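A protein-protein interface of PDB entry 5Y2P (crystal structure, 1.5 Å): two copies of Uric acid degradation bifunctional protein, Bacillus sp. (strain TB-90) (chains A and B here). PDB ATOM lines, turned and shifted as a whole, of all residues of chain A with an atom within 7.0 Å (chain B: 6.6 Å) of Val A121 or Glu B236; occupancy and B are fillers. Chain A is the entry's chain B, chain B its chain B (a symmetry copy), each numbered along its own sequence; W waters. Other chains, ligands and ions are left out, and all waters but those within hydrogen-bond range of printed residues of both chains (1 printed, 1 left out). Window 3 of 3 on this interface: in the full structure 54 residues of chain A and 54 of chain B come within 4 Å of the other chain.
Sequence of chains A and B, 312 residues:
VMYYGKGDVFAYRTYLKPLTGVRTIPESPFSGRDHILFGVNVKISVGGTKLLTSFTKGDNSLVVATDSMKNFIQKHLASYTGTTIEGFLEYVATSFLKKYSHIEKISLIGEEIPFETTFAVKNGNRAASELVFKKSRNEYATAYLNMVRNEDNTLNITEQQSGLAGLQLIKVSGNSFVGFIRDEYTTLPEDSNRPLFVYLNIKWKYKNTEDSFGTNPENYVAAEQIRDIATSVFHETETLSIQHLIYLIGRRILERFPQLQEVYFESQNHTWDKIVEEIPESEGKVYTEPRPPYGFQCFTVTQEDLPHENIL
Among the printed residues, pairs that only touch across the chains: Phe A119 with Asp B228 (3.8 Å), Ala A120 with Ser B232 (3.4 Å), Ala A120 with His B235 (3.5 Å), Val A121 with Pro B26 (3.6 Å), Val A121 with Glu B27 (3.8 Å), Val A121 with Glu B236 (3.6 Å), Arg A126 with Glu B27 (3.4 Å), Arg A126 with Ser B28 (3.5 Å), Leu A131 with Lys B171 (3.2 Å), Val A132 with Lys B171 (3.8 Å) and Val A132 with His B235 (3.6 Å).
The backbone NH (N) of Ala A120 lies within hydrogen-bond range of the backbone carbonyl oxygen (O) of Ala A127 (2.9 Å).
The side-chain carboxylate of Glu B27 lies within salt-bridge range of the guanidinium group of Arg B252.
The side-chain hydroxyl (OG) of Ser B28 sits at hydrogen-bond distance from the side-chain carboxylate (OD2) of Asp B228 (2.7 Å).
The side-chain amino group of Lys B171 is in hydrogen-bond range of the backbone carbonyl oxygen of His B235 (3.3 Å).
The backbone carbonyl oxygen (O) of Thr B237 lies within hydrogen-bond range of the side-chain amino group (NZ) of Lys B171 (2.6 Å).
OE1 of Glu B236 lies within salt-bridge range of NH2 of Arg B252.
O of Phe A119 sits at hydrogen-bond distance from OG1 of Thr B231 (2.7 Å).
O of Phe A119 lies within hydrogen-bond range of N of Ser B232 (3.3 Å).
N of Val A121 lies within hydrogen-bond range of OG of Ser B232.
NH1 of Arg A126 is in hydrogen-bond range of O of Pro B26 (2.9 Å).
Water W1 lies within hydrogen-bond range of the side-chain hydroxyl of Thr B231 (2.6 Å), the side-chain carboxylate of Asp B228 (2.8 Å) and the backbone NH of Phe A119 (3.1 Å).
Of chain B, only Pro B26, Glu B27, Ser B232 and Glu B236 come within 4 Å of Val A121.
Printed residues of chain A within 4 Å of Asp B228: Phe A119 (3.8 Å).
Of the printed residues of chain B, Leu A131 touches Lys B171 (3.2 Å).
Of the printed residues of chain A, Glu B27 touches Val A121 and Arg A126.
Val B233 touches none of the printed residues of chain A.
The nearest residue of chain B that does not touch Val A121 is His B235 (5.1 Å).
The nearest residue of chain A that does not touch Glu B236 is Ala A120 (5.4 Å).
The nearest printed residue of chain A that does not touch Glu B27 is Phe A119 (4.2 Å).
Of the 11 printed residues of chain A, 6 touch a printed residue of chain B.
Printed residues of chain A that touch a printed residue of chain B: Phe A119, Ala A120, Val A121, Arg A126, Leu A131 and Val A132.
Hydrophobic or aromatic side chains of chain B within 4 Å of the printed part of chain A: His B235.
Among the printed residues, no Asp or Glu carboxylate lies within 4 Å of a Lys or Arg side-chain nitrogen of the other chain.
No position is printed for both chains.
Of the 15 pairs that touch across the chains among the printed residues, none has its exchanged pair printed and touching as well.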
ATOM      1  N   PHE A 119       0.170  21.472  -9.636  1.00  0.00           N
ATOM      2  CA  PHE A 119      -0.587  22.136 -10.688  1.00  0.00           C
ATOM      3  C   PHE A 119       0.346  22.806 -11.674  1.00  0.00           C
ATOM      4  O   PHE A 119       1.375  23.363 -11.294  1.00  0.00           O
ATOM      5  CB  PHE A 119      -1.489  23.246 -10.116  1.00  0.00           C
ATOM      6  CG  PHE A 119      -2.644  22.745  -9.302  1.00  0.00           C
ATOM      7  CD1 PHE A 119      -3.634  21.974  -9.887  1.00  0.00           C
ATOM      8  CD2 PHE A 119      -2.753  23.065  -7.962  1.00  0.00           C
ATOM      9  CE1 PHE A 119      -4.720  21.518  -9.137  1.00  0.00           C
ATOM     10  CE2 PHE A 119      -3.834  22.614  -7.210  1.00  0.00           C
ATOM     11  CZ  PHE A 119      -4.814  21.842  -7.802  1.00  0.00           C
ATOM     12  N   ALA A 120      -0.052  22.799 -12.951  1.00  0.00           N
ATOM     13  CA  ALA A 120       0.638  23.564 -13.976  1.00  0.00           C
ATOM     14  C   ALA A 120      -0.349  24.032 -15.031  1.00  0.00           C
ATOM     15  O   ALA A 120      -1.342  23.364 -15.332  1.00  0.00           O
ATOM     16  CB  ALA A 120       1.711  22.739 -14.686  1.00  0.00           C
ATOM     17  N   VAL A 121      -0.067  25.189 -15.596  1.00  0.00           N
ATOM     18  CA  VAL A 121      -0.858  25.743 -16.691  1.00  0.00           C
ATOM     19  C   VAL A 121      -0.156  25.423 -17.998  1.00  0.00           C
ATOM     20  O   VAL A 121       1.042  25.683 -18.140  1.00  0.00           O
ATOM     21  CB  VAL A 121      -1.022  27.261 -16.531  1.00  0.00           C
ATOM     22  CG1 VAL A 121      -1.799  27.858 -17.723  1.00  0.00           C
ATOM     23  CG2 VAL A 121      -1.726  27.574 -15.233  1.00  0.00           C
ATOM     24  N   LYS A 122      -0.920  24.947 -18.982  1.00  0.00           N
ATOM     25  CA  LYS A 122      -0.392  24.742 -20.333  1.00  0.00           C
ATOM     26  C   LYS A 122      -1.567  24.589 -21.283  1.00  0.00           C
ATOM     27  O   LYS A 122      -2.613  24.043 -20.916  1.00  0.00           O
ATOM     28  CB  LYS A 122       0.507  23.502 -20.394  1.00  0.00           C
ATOM     29  N   ASN A 123      -1.392  25.085 -22.505  1.00  0.00           N
ATOM     30  CA  ASN A 123      -2.386  24.913 -23.563  1.00  0.00           C
ATOM     31  C   ASN A 123      -3.743  25.518 -23.207  1.00  0.00           C
ATOM     32  O   ASN A 123      -4.768  25.154 -23.805  1.00  0.00           O
ATOM     33  CB  ASN A 123      -2.525  23.438 -23.941  1.00  0.00           C
ATOM     34  CG  ASN A 123      -1.261  22.885 -24.568  1.00  0.00           C
ATOM     35  OD1 ASN A 123      -0.799  23.378 -25.601  1.00  0.00           O
ATOM     36  ND2 ASN A 123      -0.682  21.879 -23.936  1.00  0.00           N
ATOM     37  N   GLY A 124      -3.773  26.450 -22.255  1.00  0.00           N
ATOM     38  CA  GLY A 124      -4.983  27.172 -21.925  1.00  0.00           C
ATOM     39  C   GLY A 124      -5.712  26.674 -20.694  1.00  0.00           C
ATOM     40  O   GLY A 124      -6.770  27.223 -20.366  1.00  0.00           O
ATOM     41  N   ASN A 125      -5.195  25.656 -20.015  1.00  0.00           N
ATOM     42  CA  ASN A 125      -5.851  25.126 -18.830  1.00  0.00           C
ATOM     43  C   ASN A 125      -4.830  24.679 -17.788  1.00  0.00           C
ATOM     44  O   ASN A 125      -3.690  24.301 -18.097  1.00  0.00           O
ATOM     45  CB  ASN A 125      -6.853  23.998 -19.185  1.00  0.00           C
ATOM     46  CG  ASN A 125      -6.168  22.694 -19.552  1.00  0.00           C
ATOM     47  OD1 ASN A 125      -5.313  22.651 -20.428  1.00  0.00           O
ATOM     48  ND2 ASN A 125      -6.526  21.626 -18.846  1.00  0.00           N
ATOM     49  N   ARG A 126      -5.264  24.737 -16.531  1.00  0.00           N
ATOM     50  CA  ARG A 126      -4.509  24.240 -15.398  1.00  0.00           C
ATOM     51  C   ARG A 126      -4.898  22.787 -15.157  1.00  0.00           C
ATOM     52  O   ARG A 126      -6.082  22.441 -15.171  1.00  0.00           O
ATOM     53  CB  ARG A 126      -4.829  25.083 -14.157  1.00  0.00           C
ATOM     54  CG  ARG A 126      -4.091  24.669 -12.893  1.00  0.00           C
ATOM     55  CD  ARG A 126      -4.474  25.582 -11.700  1.00  0.00           C
ATOM     56  NE  ARG A 126      -5.903  25.548 -11.360  1.00  0.00           N
ATOM     57  CZ  ARG A 126      -6.783  26.559 -11.461  1.00  0.00           C
ATOM     58  NH1 ARG A 126      -6.472  27.821 -11.844  1.00  0.00           N
ATOM     59  NH2 ARG A 126      -8.044  26.303 -11.133  1.00  0.00           N
ATOM     60  N   ALA A 127      -3.904  21.946 -14.968  1.00  0.00           N
ATOM     61  CA  ALA A 127      -4.114  20.538 -14.692  1.00  0.00           C
ATOM     62  C   ALA A 127      -2.948  20.025 -13.871  1.00  0.00           C
ATOM     63  O   ALA A 127      -1.945  20.717 -13.668  1.00  0.00           O
ATOM     64  CB  ALA A 127      -4.232  19.731 -15.985  1.00  0.00           C
ATOM     65  N   LEU A 131       4.972  15.719 -14.848  1.00  0.00           N
ATOM     66  CA  LEU A 131       6.418  15.831 -14.688  1.00  0.00           C
ATOM     67  C   LEU A 131       6.867  16.284 -13.307  1.00  0.00           C
ATOM     68  O   LEU A 131       7.930  15.849 -12.863  1.00  0.00           O
ATOM     69  CB  LEU A 131       6.959  16.826 -15.693  1.00  0.00           C
ATOM     70  CG  LEU A 131       6.703  16.514 -17.163  1.00  0.00           C
ATOM     71  CD1 LEU A 131       7.234  17.653 -17.995  1.00  0.00           C
ATOM     72  CD2 LEU A 131       7.316  15.161 -17.551  1.00  0.00           C
ATOM     73  N   VAL A 132       6.126  17.170 -12.638  1.00  0.00           N
ATOM     74  CA  VAL A 132       6.561  17.826 -11.401  1.00  0.00           C
ATOM     75  C   VAL A 132       5.757  17.280 -10.235  1.00  0.00           C
ATOM     76  O   VAL A 132       4.521  17.344 -10.239  1.00  0.00           O
ATOM     77  CB  VAL A 132       6.381  19.351 -11.472  1.00  0.00           C
ATOM     78  CG1 VAL A 132       6.781  20.015 -10.148  1.00  0.00           C
ATOM     79  CG2 VAL A 132       7.143  19.921 -12.609  1.00  0.00           C
ATOM     80  N   PRO B  26      -4.242  32.641 -12.750  1.00  0.00           N
ATOM     81  CA  PRO B  26      -4.367  31.431 -13.574  1.00  0.00           C
ATOM     82  C   PRO B  26      -3.713  30.206 -12.987  1.00  0.00           C
ATOM     83  O   PRO B  26      -4.208  29.088 -13.176  1.00  0.00           O
ATOM     84  CB  PRO B  26      -3.693  31.834 -14.882  1.00  0.00           C
ATOM     85  CG  PRO B  26      -3.860  33.302 -14.974  1.00  0.00           C
ATOM     86  CD  PRO B  26      -3.705  33.767 -13.535  1.00  0.00           C
ATOM     87  N   GLU B  27      -2.603  30.366 -12.277  1.00  0.00           N
ATOM     88  CA  GLU B  27      -1.860  29.196 -11.845  1.00  0.00           C
ATOM     89  C   GLU B  27      -2.464  28.508 -10.627  1.00  0.00           C
ATOM     90  O   GLU B  27      -1.992  27.423 -10.269  1.00  0.00           O
ATOM     91  CB  GLU B  27      -0.407  29.575 -11.518  1.00  0.00           C
ATOM     92  CG  GLU B  27       0.463  29.986 -12.721  1.00  0.00           C
ATOM     93  CD  GLU B  27       0.226  31.403 -13.252  1.00  0.00           C
ATOM     94  OE1 GLU B  27      -0.540  32.186 -12.625  1.00  0.00           O
ATOM     95  OE2 GLU B  27       0.836  31.722 -14.290  1.00  0.00           O
ATOM     96  N   SER B  28      -3.456  29.110  -9.970  1.00  0.00           N
ATOM     97  CA  SER B  28      -3.909  28.584  -8.692  1.00  0.00           C
ATOM     98  C   SER B  28      -5.422  28.559  -8.541  1.00  0.00           C
ATOM     99  O   SER B  28      -6.065  29.588  -8.750  1.00  0.00           O
ATOM    100  CB  SER B  28      -3.305  29.452  -7.577  1.00  0.00           C
ATOM    101  OG  SER B  28      -3.652  28.960  -6.290  1.00  0.00           O
ATOM    102  N   LYS B 171      11.208  17.248 -10.644  1.00  0.00           N
ATOM    103  CA  LYS B 171      10.717  17.185 -12.017  1.00  0.00           C
ATOM    104  C   LYS B 171      11.471  16.065 -12.728  1.00  0.00           C
ATOM    105  O   LYS B 171      12.702  16.114 -12.833  1.00  0.00           O
ATOM    106  CB  LYS B 171      10.909  18.519 -12.737  1.00  0.00           C
ATOM    107  CG  LYS B 171      10.307  18.511 -14.102  1.00  0.00           C
ATOM    108  CD  LYS B 171      10.574  19.846 -14.807  1.00  0.00           C
ATOM    109  CE  LYS B 171       9.947  19.840 -16.184  1.00  0.00           C
ATOM    110  NZ  LYS B 171      10.329  21.039 -16.987  1.00  0.00           N
ATOM    111  N   ASP B 228       1.719  27.425  -6.187  1.00  0.00           N
ATOM    112  CA  ASP B 228       1.192  26.952  -7.460  1.00  0.00           C
ATOM    113  C   ASP B 228       1.896  27.617  -8.638  1.00  0.00           C
ATOM    114  O   ASP B 228       2.063  27.000  -9.701  1.00  0.00           O
ATOM    115  CB  ASP B 228      -0.313  27.188  -7.503  1.00  0.00           C
ATOM    116  CG  ASP B 228      -1.073  26.299  -6.507  1.00  0.00           C
ATOM    117  OD1 ASP B 228      -0.469  25.308  -5.986  1.00  0.00           O
ATOM    118  OD2 ASP B 228      -2.234  26.625  -6.207  1.00  0.00           O
ATOM    119  N   ILE B 229       2.311  28.877  -8.488  1.00  0.00           N
ATOM    120  CA  ILE B 229       3.177  29.485  -9.492  1.00  0.00           C
ATOM    121  C   ILE B 229       4.471  28.688  -9.625  1.00  0.00           C
ATOM    122  O   ILE B 229       4.933  28.403 -10.738  1.00  0.00           O
ATOM    123  CB  ILE B 229       3.464  30.956  -9.151  1.00  0.00           C
ATOM    124  CG1 ILE B 229       2.211  31.802  -9.397  1.00  0.00           C
ATOM    125  CG2 ILE B 229       4.631  31.464 -10.024  1.00  0.00           C
ATOM    126  CD1 ILE B 229       2.331  33.256  -8.932  1.00  0.00           C
ATOM    127  N   THR B 231       5.221  25.564  -8.980  1.00  0.00           N
ATOM    128  CA  THR B 231       5.081  24.278  -9.641  1.00  0.00           C
ATOM    129  C   THR B 231       4.769  24.459 -11.118  1.00  0.00           C
ATOM    130  O   THR B 231       5.291  23.713 -11.950  1.00  0.00           O
ATOM    131  CB  THR B 231       4.046  23.407  -8.939  1.00  0.00           C
ATOM    132  OG1 THR B 231       2.756  24.010  -9.018  1.00  0.00           O
ATOM    133  CG2 THR B 231       4.450  23.175  -7.444  1.00  0.00           C
ATOM    134  N   SER B 232       3.921  25.434 -11.467  1.00  0.00           N
ATOM    135  CA  SER B 232       3.599  25.660 -12.881  1.00  0.00           C
ATOM    136  C   SER B 232       4.844  26.047 -13.667  1.00  0.00           C
ATOM    137  O   SER B 232       5.122  25.489 -14.730  1.00  0.00           O
ATOM    138  CB  SER B 232       2.515  26.738 -13.037  1.00  0.00           C
ATOM    139  OG  SER B 232       1.968  26.713 -14.350  1.00  0.00           O
ATOM    140  N   VAL B 233       5.621  27.002 -13.151  1.00  0.00           N
ATOM    141  CA  VAL B 233       6.793  27.468 -13.896  1.00  0.00           C
ATOM    142  C   VAL B 233       7.817  26.345 -14.043  1.00  0.00           C
ATOM    143  O   VAL B 233       8.451  26.191 -15.090  1.00  0.00           O
ATOM    144  CB  VAL B 233       7.382  28.713 -13.208  1.00  0.00           C
ATOM    145  CG1 VAL B 233       8.719  29.080 -13.818  1.00  0.00           C
ATOM    146  CG2 VAL B 233       6.392  29.897 -13.308  1.00  0.00           C
ATOM    147  N   PHE B 234       8.006  25.552 -12.992  1.00  0.00           N
ATOM    148  CA  PHE B 234       8.923  24.415 -13.086  1.00  0.00           C
ATOM    149  C   PHE B 234       8.483  23.463 -14.207  1.00  0.00           C
ATOM    150  O   PHE B 234       9.292  23.050 -15.052  1.00  0.00           O
ATOM    151  CB  PHE B 234       8.976  23.728 -11.707  1.00  0.00           C
ATOM    152  CG  PHE B 234      10.165  22.806 -11.451  1.00  0.00           C
ATOM    153  CD1 PHE B 234      11.191  22.616 -12.362  1.00  0.00           C
ATOM    154  CD2 PHE B 234      10.222  22.123 -10.244  1.00  0.00           C
ATOM    155  CE1 PHE B 234      12.255  21.757 -12.051  1.00  0.00           C
ATOM    156  CE2 PHE B 234      11.265  21.292  -9.944  1.00  0.00           C
ATOM    157  CZ  PHE B 234      12.293  21.112 -10.863  1.00  0.00           C
ATOM    158  N   HIS B 235       7.188  23.163 -14.274  1.00  0.00           N
ATOM    159  CA  HIS B 235       6.653  22.293 -15.317  1.00  0.00           C
ATOM    160  C   HIS B 235       6.865  22.884 -16.712  1.00  0.00           C
ATOM    161  O   HIS B 235       7.281  22.188 -17.652  1.00  0.00           O
ATOM    162  CB  HIS B 235       5.158  22.116 -15.077  1.00  0.00           C
ATOM    163  CG  HIS B 235       4.502  21.268 -16.102  1.00  0.00           C
ATOM    164  ND1 HIS B 235       4.082  21.727 -17.344  1.00  0.00           N
ATOM    165  CD2 HIS B 235       4.238  19.953 -16.087  1.00  0.00           C
ATOM    166  CE1 HIS B 235       3.564  20.717 -18.021  1.00  0.00           C
ATOM    167  NE2 HIS B 235       3.653  19.629 -17.280  1.00  0.00           N
ATOM    168  N   GLU B 236       6.560  24.174 -16.853  1.00  0.00           N
ATOM    169  CA  GLU B 236       6.578  24.860 -18.141  1.00  0.00           C
ATOM    170  C   GLU B 236       7.985  24.989 -18.718  1.00  0.00           C
ATOM    171  O   GLU B 236       8.131  25.107 -19.936  1.00  0.00           O
ATOM    172  CB  GLU B 236       6.006  26.269 -17.940  1.00  0.00           C
ATOM    173  CG  GLU B 236       4.500  26.346 -17.522  1.00  0.00           C
ATOM    174  CD  GLU B 236       4.051  27.786 -17.252  1.00  0.00           C
ATOM    175  OE1 GLU B 236       4.241  28.647 -18.144  1.00  0.00           O
ATOM    176  OE2 GLU B 236       3.557  28.070 -16.139  1.00  0.00           O
ATOM    177  N   THR B 237       9.015  25.019 -17.866  1.00  0.00           N
ATOM    178  CA  THR B 237      10.356  25.441 -18.248  1.00  0.00           C
ATOM    179  C   THR B 237      11.239  24.233 -18.524  1.00  0.00           C
ATOM    180  O   THR B 237      11.347  23.343 -17.685  1.00  0.00           O
ATOM    181  CB  THR B 237      10.984  26.249 -17.103  1.00  0.00           C
ATOM    182  OG1 THR B 237      10.153  27.382 -16.793  1.00  0.00           O
ATOM    183  CG2 THR B 237      12.401  26.711 -17.481  1.00  0.00           C
ATOM    184  N   GLU B 238      11.902  24.222 -19.676  1.00  0.00           N
ATOM    185  CA  GLU B 238      13.055  23.350 -19.841  1.00  0.00           C
ATOM    186  C   GLU B 238      14.182  24.002 -19.057  1.00  0.00           C
ATOM    187  O   GLU B 238      14.826  24.938 -19.534  1.00  0.00           O
ATOM    188  CB  GLU B 238      13.428  23.234 -21.312  1.00  0.00           C
ATOM    189  CG  GLU B 238      12.255  22.888 -22.187  1.00  0.00           C
ATOM    190  CD  GLU B 238      11.659  21.540 -21.836  1.00  0.00           C
ATOM    191  OE1 GLU B 238      12.429  20.554 -21.743  1.00  0.00           O
ATOM    192  OE2 GLU B 238      10.424  21.474 -21.646  1.00  0.00           O
ATOM    193  N   ARG B 252       7.557  35.427 -12.735  1.00  0.00           N
ATOM    194  CA  ARG B 252       6.132  35.134 -12.828  1.00  0.00           C
ATOM    195  C   ARG B 252       5.389  35.645 -11.605  1.00  0.00           C
ATOM    196  O   ARG B 252       4.294  36.205 -11.727  1.00  0.00           O
ATOM    197  CB  ARG B 252       5.908  33.630 -13.013  1.00  0.00           C
ATOM    198  CG  ARG B 252       4.445  33.224 -13.177  1.00  0.00           C
ATOM    199  CD  ARG B 252       3.846  33.638 -14.518  1.00  0.00           C
ATOM    200  NE  ARG B 252       4.575  32.954 -15.583  1.00  0.00           N
ATOM    201  CZ  ARG B 252       4.362  31.692 -15.953  1.00  0.00           C
ATOM    202  NH1 ARG B 252       3.400  30.955 -15.397  1.00  0.00           N
ATOM    203  NH2 ARG B 252       5.139  31.156 -16.882  1.00  0.00           N
HETATM  204  O   HOH W   1       1.015  23.222  -7.198  1.00  0.00           O
